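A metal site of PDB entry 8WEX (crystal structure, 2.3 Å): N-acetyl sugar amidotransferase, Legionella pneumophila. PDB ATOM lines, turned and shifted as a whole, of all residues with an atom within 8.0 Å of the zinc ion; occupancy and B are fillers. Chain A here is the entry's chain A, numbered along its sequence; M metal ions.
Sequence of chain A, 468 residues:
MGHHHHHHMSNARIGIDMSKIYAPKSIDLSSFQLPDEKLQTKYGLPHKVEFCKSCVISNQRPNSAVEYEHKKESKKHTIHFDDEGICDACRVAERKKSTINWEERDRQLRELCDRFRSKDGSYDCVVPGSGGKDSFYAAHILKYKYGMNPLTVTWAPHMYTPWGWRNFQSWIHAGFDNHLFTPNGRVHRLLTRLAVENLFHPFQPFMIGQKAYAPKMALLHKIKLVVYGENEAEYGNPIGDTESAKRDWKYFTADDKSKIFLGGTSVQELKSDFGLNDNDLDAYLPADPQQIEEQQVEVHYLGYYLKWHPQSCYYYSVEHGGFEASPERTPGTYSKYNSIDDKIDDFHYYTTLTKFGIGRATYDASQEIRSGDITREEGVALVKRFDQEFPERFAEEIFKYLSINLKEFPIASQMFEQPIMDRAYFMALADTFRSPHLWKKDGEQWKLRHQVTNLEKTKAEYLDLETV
Merely in contact with the zinc ion: Arg 370 (3.5 Å).
Five residues have an atom within 4 Å of the zinc ion: Cys 52, Cys 55, Cys 87, Cys 90 and Arg 370.
The nearest printed residue that does not touch the zinc ion is Ser 54 (4.4 Å).
The zinc ion is bound by SG of Cys 87, SG of Cys 55, SG of Cys 90 and SG of Cys 52.
NH2 of Arg 370 sits close to SG of Cys 87 (3.3 Å).
The side-chain sulfur (SG) of Cys 87 lies close to the backbone NH (N) of Ala 89, 3.7 Å away.
SG of Cys 55 sits close to NH2 of Arg 370 (3.0 Å).
O of Cys 55 lies within hydrogen-bond range of NE of Arg 376, at 3.0 Å.
SG of Cys 90 lies close to NE of Arg 370 (3.4 Å).
N of Ser 54 sits close to SG of Cys 52, 3.3 Å away.
The backbone NH of Cys 52 sits at hydrogen-bond distance from the backbone carbonyl oxygen of Ile 57, at 3.0 Å.
The backbone carbonyl oxygen of Cys 52 is in hydrogen-bond range of the guanidinium group of Arg 376.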
ATOM      1  N   PHE A  51       5.781   3.506  -5.226  1.00  0.00           N
ATOM      2  CA  PHE A  51       7.253   3.671  -5.230  1.00  0.00           C
ATOM      3  C   PHE A  51       7.829   2.838  -6.369  1.00  0.00           C
ATOM      4  O   PHE A  51       7.346   1.724  -6.667  1.00  0.00           O
ATOM      5  CB  PHE A  51       7.847   3.269  -3.886  1.00  0.00           C
ATOM      6  CG  PHE A  51       7.397   4.153  -2.763  1.00  0.00           C
ATOM      7  CD1 PHE A  51       8.052   5.353  -2.515  1.00  0.00           C
ATOM      8  CD2 PHE A  51       6.298   3.828  -1.981  1.00  0.00           C
ATOM      9  CE1 PHE A  51       7.635   6.198  -1.498  1.00  0.00           C
ATOM     10  CE2 PHE A  51       5.889   4.662  -0.953  1.00  0.00           C
ATOM     11  CZ  PHE A  51       6.555   5.848  -0.718  1.00  0.00           C
ATOM     12  N   CYS A  52       8.872   3.390  -7.000  1.00  0.00           N
ATOM     13  CA  CYS A  52       9.663   2.713  -8.046  1.00  0.00           C
ATOM     14  C   CYS A  52      10.389   1.517  -7.418  1.00  0.00           C
ATOM     15  O   CYS A  52      10.778   1.631  -6.260  1.00  0.00           O
ATOM     16  CB  CYS A  52      10.631   3.698  -8.685  1.00  0.00           C
ATOM     17  SG  CYS A  52      12.046   2.950  -9.518  1.00  0.00           S
ATOM     18  N   LYS A  53      10.536   0.417  -8.159  1.00  0.00           N
ATOM     19  CA  LYS A  53      11.062  -0.871  -7.638  1.00  0.00           C
ATOM     20  C   LYS A  53      12.598  -0.932  -7.743  1.00  0.00           C
ATOM     21  O   LYS A  53      13.161  -1.902  -7.214  1.00  0.00           O
ATOM     22  CB  LYS A  53      10.399  -2.064  -8.334  1.00  0.00           C
ATOM     23  N   SER A  54      13.244   0.058  -8.352  1.00  0.00           N
ATOM     24  CA  SER A  54      14.729   0.159  -8.436  1.00  0.00           C
ATOM     25  C   SER A  54      15.256   1.169  -7.420  1.00  0.00           C
ATOM     26  O   SER A  54      16.126   0.777  -6.592  1.00  0.00           O
ATOM     27  CB  SER A  54      15.179   0.524  -9.831  1.00  0.00           C
ATOM     28  OG  SER A  54      15.402  -0.622 -10.626  1.00  0.00           O
ATOM     29  N   CYS A  55      14.799   2.440  -7.492  1.00  0.00           N
ATOM     30  CA  CYS A  55      15.176   3.491  -6.517  1.00  0.00           C
ATOM     31  C   CYS A  55      14.097   3.560  -5.433  1.00  0.00           C
ATOM     32  O   CYS A  55      13.361   2.580  -5.274  1.00  0.00           O
ATOM     33  CB  CYS A  55      15.424   4.830  -7.189  1.00  0.00           C
ATOM     34  SG  CYS A  55      13.971   5.533  -7.981  1.00  0.00           S
ATOM     35  N   VAL A  56      14.064   4.640  -4.659  1.00  0.00           N
ATOM     36  CA  VAL A  56      13.113   4.744  -3.525  1.00  0.00           C
ATOM     37  C   VAL A  56      12.223   5.953  -3.740  1.00  0.00           C
ATOM     38  O   VAL A  56      11.551   6.391  -2.786  1.00  0.00           O
ATOM     39  CB  VAL A  56      13.852   4.811  -2.178  1.00  0.00           C
ATOM     40  CG1 VAL A  56      14.391   3.440  -1.792  1.00  0.00           C
ATOM     41  CG2 VAL A  56      14.968   5.851  -2.185  1.00  0.00           C
ATOM     42  N   ILE A  57      12.191   6.469  -4.966  1.00  0.00           N
ATOM     43  CA  ILE A  57      11.350   7.662  -5.260  1.00  0.00           C
ATOM     44  C   ILE A  57       9.929   7.183  -5.550  1.00  0.00           C
ATOM     45  O   ILE A  57       9.750   6.010  -5.908  1.00  0.00           O
ATOM     46  CB  ILE A  57      11.893   8.525  -6.405  1.00  0.00           C
ATOM     47  CG1 ILE A  57      11.427   9.970  -6.221  1.00  0.00           C
ATOM     48  CG2 ILE A  57      11.470   7.962  -7.752  1.00  0.00           C
ATOM     49  CD1 ILE A  57      12.212  10.990  -6.965  1.00  0.00           C
ATOM     50  N   SER A  58       8.975   8.099  -5.423  1.00  0.00           N
ATOM     51  CA  SER A  58       7.547   7.842  -5.648  1.00  0.00           C
ATOM     52  C   SER A  58       7.127   8.532  -6.921  1.00  0.00           C
ATOM     53  O   SER A  58       7.907   9.324  -7.456  1.00  0.00           O
ATOM     54  CB  SER A  58       6.714   8.299  -4.478  1.00  0.00           C
ATOM     55  OG  SER A  58       6.347   9.659  -4.601  1.00  0.00           O
ATOM     56  N   PHE A  81       5.577   5.405 -14.020  1.00  0.00           N
ATOM     57  CA  PHE A  81       6.520   4.253 -14.051  1.00  0.00           C
ATOM     58  C   PHE A  81       6.193   3.330 -15.209  1.00  0.00           C
ATOM     59  O   PHE A  81       5.071   3.405 -15.744  1.00  0.00           O
ATOM     60  CB  PHE A  81       6.487   3.481 -12.727  1.00  0.00           C
ATOM     61  CG  PHE A  81       6.876   4.309 -11.532  1.00  0.00           C
ATOM     62  CD1 PHE A  81       7.569   5.500 -11.683  1.00  0.00           C
ATOM     63  CD2 PHE A  81       6.533   3.902 -10.247  1.00  0.00           C
ATOM     64  CE1 PHE A  81       7.933   6.265 -10.585  1.00  0.00           C
ATOM     65  CE2 PHE A  81       6.908   4.660  -9.147  1.00  0.00           C
ATOM     66  CZ  PHE A  81       7.595   5.832  -9.320  1.00  0.00           C
ATOM     67  N   GLY A  85       7.453  -1.394 -13.114  1.00  0.00           N
ATOM     68  CA  GLY A  85       7.388  -0.443 -11.996  1.00  0.00           C
ATOM     69  C   GLY A  85       8.726   0.228 -11.723  1.00  0.00           C
ATOM     70  O   GLY A  85       9.155   0.245 -10.552  1.00  0.00           O
ATOM     71  N   ILE A  86       9.358   0.765 -12.785  1.00  0.00           N
ATOM     72  CA  ILE A  86      10.695   1.436 -12.737  1.00  0.00           C
ATOM     73  C   ILE A  86      10.535   2.848 -13.296  1.00  0.00           C
ATOM     74  O   ILE A  86      10.080   2.966 -14.435  1.00  0.00           O
ATOM     75  CB  ILE A  86      11.774   0.631 -13.491  1.00  0.00           C
ATOM     76  CG1 ILE A  86      11.819  -0.830 -13.040  1.00  0.00           C
ATOM     77  CG2 ILE A  86      13.144   1.279 -13.389  1.00  0.00           C
ATOM     78  CD1 ILE A  86      12.020  -1.008 -11.549  1.00  0.00           C
ATOM     79  N   CYS A  87      10.873   3.859 -12.485  1.00  0.00           N
ATOM     80  CA  CYS A  87      10.941   5.279 -12.912  1.00  0.00           C
ATOM     81  C   CYS A  87      11.813   5.362 -14.170  1.00  0.00           C
ATOM     82  O   CYS A  87      12.749   4.564 -14.316  1.00  0.00           O
ATOM     83  CB  CYS A  87      11.466   6.191 -11.808  1.00  0.00           C
ATOM     84  SG  CYS A  87      13.216   5.979 -11.417  1.00  0.00           S
ATOM     85  N   ASP A  88      11.472   6.294 -15.059  1.00  0.00           N
ATOM     86  CA  ASP A  88      12.275   6.602 -16.267  1.00  0.00           C
ATOM     87  C   ASP A  88      13.711   6.931 -15.879  1.00  0.00           C
ATOM     88  O   ASP A  88      14.603   6.613 -16.670  1.00  0.00           O
ATOM     89  CB  ASP A  88      11.660   7.776 -17.041  1.00  0.00           C
ATOM     90  CG  ASP A  88      10.285   7.458 -17.608  1.00  0.00           C
ATOM     91  OD1 ASP A  88       9.998   6.266 -17.870  1.00  0.00           O
ATOM     92  OD2 ASP A  88       9.506   8.410 -17.809  1.00  0.00           O
ATOM     93  N   ALA A  89      13.931   7.514 -14.699  1.00  0.00           N
ATOM     94  CA  ALA A  89      15.278   7.939 -14.254  1.00  0.00           C
ATOM     95  C   ALA A  89      16.186   6.708 -14.062  1.00  0.00           C
ATOM     96  O   ALA A  89      17.348   6.788 -14.457  1.00  0.00           O
ATOM     97  CB  ALA A  89      15.223   8.761 -12.996  1.00  0.00           C
ATOM     98  N   CYS A  90      15.680   5.623 -13.475  1.00  0.00           N
ATOM     99  CA  CYS A  90      16.456   4.373 -13.270  1.00  0.00           C
ATOM    100  C   CYS A  90      16.756   3.730 -14.622  1.00  0.00           C
ATOM    101  O   CYS A  90      17.886   3.231 -14.802  1.00  0.00           O
ATOM    102  CB  CYS A  90      15.715   3.405 -12.355  1.00  0.00           C
ATOM    103  SG  CYS A  90      15.886   3.830 -10.604  1.00  0.00           S
ATOM    104  N   ARG A  91      15.809   3.758 -15.555  1.00  0.00           N
ATOM    105  CA  ARG A  91      15.979   3.129 -16.891  1.00  0.00           C
ATOM    106  C   ARG A  91      17.048   3.918 -17.647  1.00  0.00           C
ATOM    107  O   ARG A  91      17.914   3.259 -18.249  1.00  0.00           O
ATOM    108  CB  ARG A  91      14.652   3.036 -17.637  1.00  0.00           C
ATOM    109  CG  ARG A  91      13.717   1.970 -17.064  1.00  0.00           C
ATOM    110  CD  ARG A  91      13.734   0.649 -17.815  1.00  0.00           C
ATOM    111  NE  ARG A  91      13.491  -0.503 -16.958  1.00  0.00           N
ATOM    112  CZ  ARG A  91      14.404  -1.392 -16.587  1.00  0.00           C
ATOM    113  NH1 ARG A  91      15.670  -1.296 -16.986  1.00  0.00           N
ATOM    114  NH2 ARG A  91      14.057  -2.392 -15.797  1.00  0.00           N
ATOM    115  N   SER A 366      18.070   7.824  -3.852  1.00  0.00           N
ATOM    116  CA  SER A 366      17.723   7.395  -5.226  1.00  0.00           C
ATOM    117  C   SER A 366      18.923   7.621  -6.168  1.00  0.00           C
ATOM    118  O   SER A 366      19.229   6.737  -6.970  1.00  0.00           O
ATOM    119  CB  SER A 366      16.493   8.112  -5.733  1.00  0.00           C
ATOM    120  OG  SER A 366      15.360   7.729  -4.991  1.00  0.00           O
ATOM    121  N   ILE A 369      21.551   5.038  -5.389  1.00  0.00           N
ATOM    122  CA  ILE A 369      21.127   3.670  -5.811  1.00  0.00           C
ATOM    123  C   ILE A 369      21.457   3.520  -7.299  1.00  0.00           C
ATOM    124  O   ILE A 369      22.009   2.471  -7.678  1.00  0.00           O
ATOM    125  CB  ILE A 369      19.633   3.417  -5.524  1.00  0.00           C
ATOM    126  CG1 ILE A 369      19.375   3.285  -4.026  1.00  0.00           C
ATOM    127  CG2 ILE A 369      19.133   2.204  -6.294  1.00  0.00           C
ATOM    128  CD1 ILE A 369      17.953   3.545  -3.622  1.00  0.00           C
ATOM    129  N   ARG A 370      21.127   4.514  -8.110  1.00  0.00           N
ATOM    130  CA  ARG A 370      21.394   4.453  -9.565  1.00  0.00           C
ATOM    131  C   ARG A 370      22.912   4.409  -9.812  1.00  0.00           C
ATOM    132  O   ARG A 370      23.349   3.635 -10.685  1.00  0.00           O
ATOM    133  CB  ARG A 370      20.784   5.658 -10.277  1.00  0.00           C
ATOM    134  CG  ARG A 370      19.269   5.612 -10.290  1.00  0.00           C
ATOM    135  CD  ARG A 370      18.663   6.978 -10.533  1.00  0.00           C
ATOM    136  NE  ARG A 370      17.245   6.920 -10.212  1.00  0.00           N
ATOM    137  CZ  ARG A 370      16.543   7.934  -9.739  1.00  0.00           C
ATOM    138  NH1 ARG A 370      17.129   9.106  -9.524  1.00  0.00           N
ATOM    139  NH2 ARG A 370      15.262   7.770  -9.493  1.00  0.00           N
ATOM    140  N   ARG A 376      18.942  -0.601  -2.789  1.00  0.00           N
ATOM    141  CA  ARG A 376      17.578  -0.099  -2.529  1.00  0.00           C
ATOM    142  C   ARG A 376      17.271  -0.235  -1.044  1.00  0.00           C
ATOM    143  O   ARG A 376      16.604   0.642  -0.494  1.00  0.00           O
ATOM    144  CB  ARG A 376      16.560  -0.837  -3.388  1.00  0.00           C
ATOM    145  CG  ARG A 376      15.291  -0.053  -3.602  1.00  0.00           C
ATOM    146  CD  ARG A 376      14.172  -0.928  -4.141  1.00  0.00           C
ATOM    147  NE  ARG A 376      12.927  -0.194  -4.294  1.00  0.00           N
ATOM    148  CZ  ARG A 376      11.997  -0.060  -3.338  1.00  0.00           C
ATOM    149  NH1 ARG A 376      12.175  -0.593  -2.135  1.00  0.00           N
ATOM    150  NH2 ARG A 376      10.905   0.645  -3.586  1.00  0.00           N
HETATM  151 ZN    ZN M   1      13.756   4.680  -9.976  1.00  0.00          ZN
